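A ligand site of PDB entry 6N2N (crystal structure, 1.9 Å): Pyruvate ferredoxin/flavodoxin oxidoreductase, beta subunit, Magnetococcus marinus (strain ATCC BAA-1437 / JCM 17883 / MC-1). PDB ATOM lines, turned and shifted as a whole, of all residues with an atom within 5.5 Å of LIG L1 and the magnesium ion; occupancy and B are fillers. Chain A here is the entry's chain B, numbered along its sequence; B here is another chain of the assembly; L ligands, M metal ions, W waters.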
ATOM      1  N   THR A  24      33.193   7.353 -10.672  1.00  0.00           N
ATOM      2  CA  THR A  24      32.963   7.930  -9.348  1.00  0.00           C
ATOM      3  C   THR A  24      31.834   7.247  -8.572  1.00  0.00           C
ATOM      4  O   THR A  24      31.469   7.745  -7.494  1.00  0.00           O
ATOM      5  CB  THR A  24      32.652   9.414  -9.501  1.00  0.00           C
ATOM      6  OG1 THR A  24      31.468   9.563 -10.300  1.00  0.00           O
ATOM      7  CG2 THR A  24      33.794  10.136 -10.189  1.00  0.00           C
ATOM      8  N   TRP A  25      31.325   6.108  -9.030  1.00  0.00           N
ATOM      9  CA  TRP A  25      30.279   5.413  -8.284  1.00  0.00           C
ATOM     10  C   TRP A  25      30.829   4.805  -7.002  1.00  0.00           C
ATOM     11  O   TRP A  25      32.022   4.493  -6.891  1.00  0.00           O
ATOM     12  CB  TRP A  25      29.631   4.321  -9.145  1.00  0.00           C
ATOM     13  CG  TRP A  25      28.790   4.837 -10.298  1.00  0.00           C
ATOM     14  CD1 TRP A  25      27.951   5.914 -10.291  1.00  0.00           C
ATOM     15  CD2 TRP A  25      28.724   4.279 -11.624  1.00  0.00           C
ATOM     16  NE1 TRP A  25      27.363   6.071 -11.528  1.00  0.00           N
ATOM     17  CE2 TRP A  25      27.809   5.075 -12.366  1.00  0.00           C
ATOM     18  CE3 TRP A  25      29.325   3.188 -12.245  1.00  0.00           C
ATOM     19  CZ2 TRP A  25      27.504   4.807 -13.702  1.00  0.00           C
ATOM     20  CZ3 TRP A  25      29.021   2.932 -13.573  1.00  0.00           C
ATOM     21  CH2 TRP A  25      28.118   3.733 -14.281  1.00  0.00           C
ATOM     22  N   CYS A  26      29.942   4.617  -6.030  1.00  0.00           N
ATOM     23  CA  CYS A  26      30.314   4.023  -4.753  1.00  0.00           C
ATOM     24  C   CYS A  26      30.896   2.622  -4.980  1.00  0.00           C
ATOM     25  O   CYS A  26      30.515   1.929  -5.933  1.00  0.00           O
ATOM     26  CB  CYS A  26      29.104   3.905  -3.829  1.00  0.00           C
ATOM     27  SG  CYS A  26      28.258   5.459  -3.403  1.00  0.00           S
ATOM     28  N   CYS A  29      28.650  -0.524  -5.957  1.00  0.00           N
ATOM     29  CA  CYS A  29      27.477  -0.087  -6.704  1.00  0.00           C
ATOM     30  C   CYS A  29      27.252  -0.996  -7.906  1.00  0.00           C
ATOM     31  O   CYS A  29      28.191  -1.355  -8.618  1.00  0.00           O
ATOM     32  CB  CYS A  29      27.647   1.363  -7.169  1.00  0.00           C
ATOM     33  SG  CYS A  29      26.286   2.004  -8.219  1.00  0.00           S
ATOM     34  N   GLY A  30      25.992  -1.394  -8.112  1.00  0.00           N
ATOM     35  CA  GLY A  30      25.690  -2.278  -9.223  1.00  0.00           C
ATOM     36  C   GLY A  30      25.944  -1.668 -10.588  1.00  0.00           C
ATOM     37  O   GLY A  30      26.130  -2.406 -11.560  1.00  0.00           O
ATOM     38  N   HIS A  31      25.965  -0.342 -10.685  1.00  0.00           N
ATOM     39  CA  HIS A  31      26.161   0.292 -11.986  1.00  0.00           C
ATOM     40  C   HIS A  31      27.479  -0.122 -12.642  1.00  0.00           C
ATOM     41  O   HIS A  31      27.582  -0.076 -13.869  1.00  0.00           O
ATOM     42  CB  HIS A  31      26.093   1.818 -11.855  1.00  0.00           C
ATOM     43  CG  HIS A  31      24.768   2.338 -11.396  1.00  0.00           C
ATOM     44  ND1 HIS A  31      23.617   1.584 -11.410  1.00  0.00           N
ATOM     45  CD2 HIS A  31      24.414   3.551 -10.882  1.00  0.00           C
ATOM     46  CE1 HIS A  31      22.607   2.309 -10.937  1.00  0.00           C
ATOM     47  NE2 HIS A  31      23.067   3.506 -10.617  1.00  0.00           N
ATOM     48  N   CYS A  60      22.608   8.822 -10.679  1.00  0.00           N
ATOM     49  CA  CYS A  60      23.861   8.060 -10.662  1.00  0.00           C
ATOM     50  C   CYS A  60      23.981   7.212 -11.916  1.00  0.00           C
ATOM     51  O   CYS A  60      25.022   7.197 -12.582  1.00  0.00           O
ATOM     52  CB  CYS A  60      23.933   7.166  -9.418  1.00  0.00           C
ATOM     53  SG  CYS A  60      24.163   8.051  -7.852  1.00  0.00           S
ATOM     54  N   GLY A 101      18.257   5.638 -14.700  1.00  0.00           N
ATOM     55  CA  GLY A 101      17.765   4.886 -13.574  1.00  0.00           C
ATOM     56  C   GLY A 101      16.249   4.778 -13.535  1.00  0.00           C
ATOM     57  O   GLY A 101      15.533   5.217 -14.429  1.00  0.00           O
ATOM     58  N   ASP A 102      15.761   4.165 -12.452  1.00  0.00           N
ATOM     59  CA  ASP A 102      14.330   3.916 -12.348  1.00  0.00           C
ATOM     60  C   ASP A 102      13.530   5.200 -12.138  1.00  0.00           C
ATOM     61  O   ASP A 102      12.407   5.322 -12.645  1.00  0.00           O
ATOM     62  CB  ASP A 102      14.055   2.900 -11.227  1.00  0.00           C
ATOM     63  CG  ASP A 102      14.939   3.111  -9.989  1.00  0.00           C
ATOM     64  OD1 ASP A 102      16.148   3.394 -10.115  1.00  0.00           O
ATOM     65  OD2 ASP A 102      14.396   2.975  -8.875  1.00  0.00           O
ATOM     66  N   GLY A 103      14.088   6.180 -11.415  1.00  0.00           N
ATOM     67  CA  GLY A 103      13.376   7.428 -11.237  1.00  0.00           C
ATOM     68  C   GLY A 103      13.407   8.312 -12.473  1.00  0.00           C
ATOM     69  O   GLY A 103      12.374   8.853 -12.906  1.00  0.00           O
ATOM     70  N   MET A 128      18.738   1.074 -15.341  1.00  0.00           N
ATOM     71  CA  MET A 128      19.497   0.534 -14.222  1.00  0.00           C
ATOM     72  C   MET A 128      18.652   0.681 -12.958  1.00  0.00           C
ATOM     73  O   MET A 128      18.625   1.738 -12.337  1.00  0.00           O
ATOM     74  CB  MET A 128      20.836   1.249 -14.117  1.00  0.00           C
ATOM     75  CG  MET A 128      21.517   1.382 -15.466  1.00  0.00           C
ATOM     76  SD  MET A 128      23.205   1.986 -15.359  1.00  0.00           S
ATOM     77  CE  MET A 128      23.361   2.711 -16.968  1.00  0.00           C
ATOM     78  N   ASP A 129      17.987  -0.408 -12.587  1.00  0.00           N
ATOM     79  CA  ASP A 129      16.923  -0.392 -11.583  1.00  0.00           C
ATOM     80  C   ASP A 129      17.528  -0.719 -10.224  1.00  0.00           C
ATOM     81  O   ASP A 129      17.849  -1.878  -9.956  1.00  0.00           O
ATOM     82  CB  ASP A 129      15.844  -1.397 -11.975  1.00  0.00           C
ATOM     83  CG  ASP A 129      14.665  -1.418 -11.009  1.00  0.00           C
ATOM     84  OD1 ASP A 129      14.636  -0.607 -10.065  1.00  0.00           O
ATOM     85  OD2 ASP A 129      13.779  -2.285 -11.192  1.00  0.00           O
ATOM     86  N   ASN A 130      17.682   0.294  -9.363  1.00  0.00           N
ATOM     87  CA  ASN A 130      18.176   0.075  -8.011  1.00  0.00           C
ATOM     88  C   ASN A 130      17.099   0.293  -6.945  1.00  0.00           C
ATOM     89  O   ASN A 130      17.407   0.246  -5.757  1.00  0.00           O
ATOM     90  CB  ASN A 130      19.411   0.947  -7.701  1.00  0.00           C
ATOM     91  CG  ASN A 130      19.176   2.421  -7.929  1.00  0.00           C
ATOM     92  OD1 ASN A 130      18.039   2.868  -8.078  1.00  0.00           O
ATOM     93  ND2 ASN A 130      20.274   3.186  -7.942  1.00  0.00           N
ATOM     94  N   GLY A 131      15.851   0.509  -7.361  1.00  0.00           N
ATOM     95  CA  GLY A 131      14.758   0.627  -6.418  1.00  0.00           C
ATOM     96  C   GLY A 131      14.814   1.850  -5.527  1.00  0.00           C
ATOM     97  O   GLY A 131      14.250   1.824  -4.431  1.00  0.00           O
ATOM     98  N   ILE A 132      15.474   2.913  -5.966  1.00  0.00           N
ATOM     99  CA  ILE A 132      15.670   4.099  -5.137  1.00  0.00           C
ATOM    100  C   ILE A 132      16.175   5.252  -5.998  1.00  0.00           C
ATOM    101  O   ILE A 132      16.608   5.041  -7.138  1.00  0.00           O
ATOM    102  CB  ILE A 132      16.632   3.783  -3.975  1.00  0.00           C
ATOM    103  CG1 ILE A 132      16.395   4.728  -2.789  1.00  0.00           C
ATOM    104  CG2 ILE A 132      18.084   3.811  -4.445  1.00  0.00           C
ATOM    105  CD1 ILE A 132      16.934   4.207  -1.472  1.00  0.00           C
ATOM    106  N   TYR A 133      16.112   6.482  -5.472  1.00  0.00           N
ATOM    107  CA  TYR A 133      16.812   7.623  -6.076  1.00  0.00           C
ATOM    108  C   TYR A 133      18.175   7.732  -5.400  1.00  0.00           C
ATOM    109  O   TYR A 133      18.281   8.229  -4.281  1.00  0.00           O
ATOM    110  CB  TYR A 133      16.035   8.914  -5.896  1.00  0.00           C
ATOM    111  CG  TYR A 133      14.651   8.975  -6.512  1.00  0.00           C
ATOM    112  CD1 TYR A 133      14.214   8.003  -7.402  1.00  0.00           C
ATOM    113  CD2 TYR A 133      13.786  10.022  -6.211  1.00  0.00           C
ATOM    114  CE1 TYR A 133      12.936   8.077  -7.964  1.00  0.00           C
ATOM    115  CE2 TYR A 133      12.517  10.105  -6.763  1.00  0.00           C
ATOM    116  CZ  TYR A 133      12.103   9.119  -7.633  1.00  0.00           C
ATOM    117  OH  TYR A 133      10.846   9.210  -8.184  1.00  0.00           O
ATOM    118  N   GLY A 134      19.213   7.299  -6.108  1.00  0.00           N
ATOM    119  CA  GLY A 134      20.555   7.340  -5.523  1.00  0.00           C
ATOM    120  C   GLY A 134      21.130   8.738  -5.474  1.00  0.00           C
ATOM    121  O   GLY A 134      21.571   9.200  -4.413  1.00  0.00           O
ATOM    122  N   LEU A 135      21.128   9.441  -6.609  1.00  0.00           N
ATOM    123  CA  LEU A 135      21.908  10.670  -6.726  1.00  0.00           C
ATOM    124  C   LEU A 135      21.395  11.755  -5.781  1.00  0.00           C
ATOM    125  O   LEU A 135      22.192  12.538  -5.250  1.00  0.00           O
ATOM    126  CB  LEU A 135      21.923  11.179  -8.162  1.00  0.00           C
ATOM    127  CG  LEU A 135      22.817  12.395  -8.409  1.00  0.00           C
ATOM    128  CD1 LEU A 135      24.277  12.087  -8.052  1.00  0.00           C
ATOM    129  CD2 LEU A 135      22.707  12.880  -9.846  1.00  0.00           C
ATOM    130  N   SER A 141      11.430   5.222  -5.118  1.00  0.00           N
ATOM    131  CA  SER A 141      11.191   5.276  -6.549  1.00  0.00           C
ATOM    132  C   SER A 141       9.960   4.459  -6.896  1.00  0.00           C
ATOM    133  O   SER A 141       9.397   3.763  -6.042  1.00  0.00           O
ATOM    134  CB  SER A 141      12.419   4.731  -7.293  1.00  0.00           C
ATOM    135  OG  SER A 141      12.355   3.321  -7.428  1.00  0.00           O
ATOM    136  N   GLN A 208      22.421  -2.975  -7.568  1.00  0.00           N
ATOM    137  CA  GLN A 208      22.328  -2.647  -6.155  1.00  0.00           C
ATOM    138  C   GLN A 208      22.835  -1.228  -5.882  1.00  0.00           C
ATOM    139  O   GLN A 208      23.797  -0.757  -6.503  1.00  0.00           O
ATOM    140  CB  GLN A 208      23.102  -3.666  -5.313  1.00  0.00           C
ATOM    141  CG  GLN A 208      24.618  -3.637  -5.510  1.00  0.00           C
ATOM    142  CD  GLN A 208      25.091  -4.517  -6.647  1.00  0.00           C
ATOM    143  OE1 GLN A 208      24.282  -5.070  -7.404  1.00  0.00           O
ATOM    144  NE2 GLN A 208      26.406  -4.658  -6.787  1.00  0.00           N
ATOM    145  N   CYS A 209      22.155  -0.548  -4.959  1.00  0.00           N
ATOM    146  CA  CYS A 209      22.641   0.702  -4.380  1.00  0.00           C
ATOM    147  C   CYS A 209      22.911   0.433  -2.907  1.00  0.00           C
ATOM    148  O   CYS A 209      22.025   0.613  -2.061  1.00  0.00           O
ATOM    149  CB  CYS A 209      21.636   1.846  -4.543  1.00  0.00           C
ATOM    150  SG  CYS A 209      22.097   3.358  -3.654  1.00  0.00           S
ATOM    151  N   PRO A 210      24.114  -0.041  -2.550  1.00  0.00           N
ATOM    152  CA  PRO A 210      24.367  -0.372  -1.137  1.00  0.00           C
ATOM    153  C   PRO A 210      24.334   0.832  -0.219  1.00  0.00           C
ATOM    154  O   PRO A 210      24.005   0.687   0.962  1.00  0.00           O
ATOM    155  CB  PRO A 210      25.765  -1.011  -1.176  1.00  0.00           C
ATOM    156  CG  PRO A 210      26.418  -0.404  -2.378  1.00  0.00           C
ATOM    157  CD  PRO A 210      25.299  -0.273  -3.392  1.00  0.00           C
ATOM    158  N   THR A 211      24.613   2.028  -0.750  1.00  0.00           N
ATOM    159  CA  THR A 211      24.748   3.218   0.106  1.00  0.00           C
ATOM    160  C   THR A 211      23.401   3.634   0.689  1.00  0.00           C
ATOM    161  O   THR A 211      23.332   4.048   1.856  1.00  0.00           O
ATOM    162  CB  THR A 211      25.370   4.360  -0.690  1.00  0.00           C
ATOM    163  OG1 THR A 211      26.668   3.973  -1.166  1.00  0.00           O
ATOM    164  CG2 THR A 211      25.540   5.598   0.191  1.00  0.00           C
ATOM    165  N   PHE A 212      22.317   3.549  -0.098  1.00  0.00           N
ATOM    166  CA  PHE A 212      21.007   4.002   0.364  1.00  0.00           C
ATOM    167  C   PHE A 212      19.938   2.913   0.410  1.00  0.00           C
ATOM    168  O   PHE A 212      19.071   2.973   1.276  1.00  0.00           O
ATOM    169  CB  PHE A 212      20.494   5.165  -0.512  1.00  0.00           C
ATOM    170  CG  PHE A 212      21.369   6.381  -0.462  1.00  0.00           C
ATOM    171  CD1 PHE A 212      21.448   7.151   0.683  1.00  0.00           C
ATOM    172  CD2 PHE A 212      22.133   6.741  -1.560  1.00  0.00           C
ATOM    173  CE1 PHE A 212      22.265   8.269   0.739  1.00  0.00           C
ATOM    174  CE2 PHE A 212      22.955   7.865  -1.516  1.00  0.00           C
ATOM    175  CZ  PHE A 212      23.020   8.631  -0.362  1.00  0.00           C
ATOM    176  N   ILE B  46      29.097  11.077  -3.618  1.00  0.00           N
ATOM    177  CA  ILE B  46      28.435  10.384  -2.520  1.00  0.00           C
ATOM    178  C   ILE B  46      29.392   9.394  -1.858  1.00  0.00           C
ATOM    179  O   ILE B  46      29.388   9.232  -0.625  1.00  0.00           O
ATOM    180  CB  ILE B  46      27.167   9.678  -3.041  1.00  0.00           C
ATOM    181  CG1 ILE B  46      26.133  10.721  -3.491  1.00  0.00           C
ATOM    182  CG2 ILE B  46      26.612   8.721  -2.006  1.00  0.00           C
ATOM    183  CD1 ILE B  46      24.859  10.132  -4.071  1.00  0.00           C
HETATM  184 FE1  LIG L   1      23.782   4.277  -4.873  1.00  0.00          FE
HETATM  185 FE2  LIG L   1      25.625   3.664  -6.812  1.00  0.00          FE
HETATM  186 FE3  LIG L   1      24.693   6.226  -6.560  1.00  0.00          FE
HETATM  187 FE4  LIG L   1      26.378   5.180  -4.680  1.00  0.00          FE
HETATM  188  S1  LIG L   1      26.866   5.577  -6.869  1.00  0.00           S
HETATM  189  S2  LIG L   1      24.459   6.376  -4.308  1.00  0.00           S
HETATM  190  S3  LIG L   1      25.690   3.014  -4.624  1.00  0.00           S
HETATM  191  S4  LIG L   1      23.474   4.374  -7.130  1.00  0.00           S
HETATM  192  N1  LG2 L   2      13.731  17.491 -10.957  1.00  0.00           N
HETATM  193  C1  LG2 L   2      14.323  17.976 -12.028  1.00  0.00           C
HETATM  194  C2  LG2 L   2      13.473  18.737 -13.066  1.00  0.00           C
HETATM  195  N2  LG2 L   2      15.611  17.805 -12.240  1.00  0.00           N
HETATM  196  C3  LG2 L   2      16.382  17.143 -11.350  1.00  0.00           C
HETATM  197  N3  LG2 L   2      17.776  16.992 -11.607  1.00  0.00           N
HETATM  198  C4  LG2 L   2      15.792  16.601 -10.196  1.00  0.00           C
HETATM  199  C5  LG2 L   2      14.408  16.816 -10.021  1.00  0.00           C
HETATM  200  C6  LG2 L   2      16.607  15.823  -9.097  1.00  0.00           C
HETATM  201  N4  LG2 L   2      17.037  14.497  -9.395  1.00  0.00           N
HETATM  202  C7  LG2 L   2      18.274  14.139  -9.927  1.00  0.00           C
HETATM  203  S1  LG2 L   2      18.587  12.550 -10.128  1.00  0.00           S
HETATM  204  C8  LG2 L   2      17.106  12.243  -9.513  1.00  0.00           C
HETATM  205  C9  LG2 L   2      16.347  13.349  -9.130  1.00  0.00           C
HETATM  206  C10 LG2 L   2      14.947  13.260  -8.531  1.00  0.00           C
HETATM  207  C11 LG2 L   2      16.624  10.805  -9.376  1.00  0.00           C
HETATM  208  C12 LG2 L   2      17.779   9.762  -9.402  1.00  0.00           C
HETATM  209  O1  LG2 L   2      17.174   8.459  -9.315  1.00  0.00           O
HETATM  210  P1  LG2 L   2      17.420   7.422 -10.470  1.00  0.00           P
HETATM  211  O2  LG2 L   2      16.923   7.928 -11.793  1.00  0.00           O
HETATM  212  O3  LG2 L   2      16.698   6.148 -10.098  1.00  0.00           O
HETATM  213  O4  LG2 L   2      18.970   7.166 -10.688  1.00  0.00           O
HETATM  214  P2  LG2 L   2      19.985   6.606  -9.576  1.00  0.00           P
HETATM  215  O5  LG2 L   2      20.952   5.735 -10.325  1.00  0.00           O
HETATM  216  O6  LG2 L   2      19.187   5.845  -8.543  1.00  0.00           O
HETATM  217  O7  LG2 L   2      20.688   7.770  -8.928  1.00  0.00           O
HETATM  218 MG    MG M   1      17.552   4.595  -9.038  1.00  0.00          MG
HETATM  219  O   HOH W   1      22.794   1.380  -8.030  1.00  0.00           O
HETATM  220  O   HOH W   2      18.764   3.823 -10.544  1.00  0.00           O
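The side-chain sulfur of Cys 60 binds an iron atom (FE3) of LIG L1, 2.3 Å away.
The side-chain sulfur (SG) of Cys 209 is bound to an iron atom (FE1) of LIG L1, 2.3 Å away.
The side-chain amide nitrogen of Asn 130 sits close to a sulfur (S4) of LIG L1 (3.5 Å).
A sulfur (S1) of LIG L1 sits close to the backbone NH (N) of Cys 26.
An oxygen (O5) of LG2 L2 is in hydrogen-bond range of a ring nitrogen (NE2) of His 31, at 3.1 Å.
The backbone NH of Leu 135 is in hydrogen-bond range of an oxygen (O7) of LG2 L2 (2.9 Å).
SG of Cys 29 binds FE2 of LIG L1, 2.3 Å away.
The backbone NH of Gly 134 lies within hydrogen-bond range of an oxygen (O7) of LG2 L2.
SG of Cys 60 lies close to O7 of LG2 L2, at 3.6 Å.
An oxygen (O2) of LG2 L2 is in hydrogen-bond range of the backbone NH (N) of Gly 103.
S4 of LIG L1 lies close to NE2 of His 31 (3.6 Å).
N of Asp 102 lies close to O3 of LG2 L2.
A sulfur (S3) of LIG L1 sits close to the side-chain hydroxyl (OG1) of Thr 211.
O7 of LG2 L2 lies within hydrogen-bond range of N of Cys 60 (2.8 Å).
SG of Cys 26 binds FE4 of LIG L1, 2.3 Å away.
The backbone carbonyl oxygen (O) of Cys 60 sits at hydrogen-bond distance from the indole nitrogen (NE1) of Trp 25 (2.8 Å).
The side-chain hydroxyl of Ser 141 is in hydrogen-bond range of the side-chain carboxylate of Asp 102 (2.5 Å).
SG of Cys 60 sits close to N of Leu 135 (3.6 Å).
The side-chain hydroxyl of Thr 211 sits close to the side-chain sulfur of Cys 26 (3.1 Å).
The side-chain sulfur of Cys 209 sits close to the backbone NH of Phe 212 (3.6 Å).
The backbone NH (N) of Gly 131 sits at hydrogen-bond distance from the side-chain carboxylate (OD2) of Asp 102, 3.2 Å away.
SG of Cys 29 lies close to N of His 31, 3.4 Å away.
N of Ile 132 sits at hydrogen-bond distance from OG of Ser 141, 3.5 Å away.
Residues that only touch LIG L1: Trp 25 (3.6 Å), Pro 210 (3.5 Å), Phe 212 (3.5 Å) and Ile 46 of chain B (3.8 Å).
11 residues have an atom within 4 Å of LIG L1: Trp 25, Cys 26, Cys 29, His 31, Cys 60, Asn 130, Cys 209, Pro 210, Thr 211, Phe 212 and Ile 46 of chain B.
The nearest printed residue that does not touch LIG L1 is Gly 134 (4.04 Å).
Along chain A the residues within 4 Å of the magnesium ion span positions 102 to 132.
The nearest printed residue that does not touch the magnesium ion is Tyr 133 (4.3 Å).
The magnesium ion is bound by OD1 of Asn 130, O3 of LG2 L2, water W2, O6 of LG2 L2, OD1 of Asp 102 and O of Ile 132.
The magnesium ion has six donor atoms within binding distance.
Water W2 lies within hydrogen-bond range of the backbone carbonyl oxygen (O) of Met 128 (2.8 Å), an oxygen (O5) of LG2 L2 (2.9 Å) and the side-chain amide nitrogen (ND2) of Asn 130 (3.1 Å).
Water W1 lies within hydrogen-bond range of O of Gln 208, ND2 of Asn 130, S4 of LIG L1 and NE2 of His 31.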
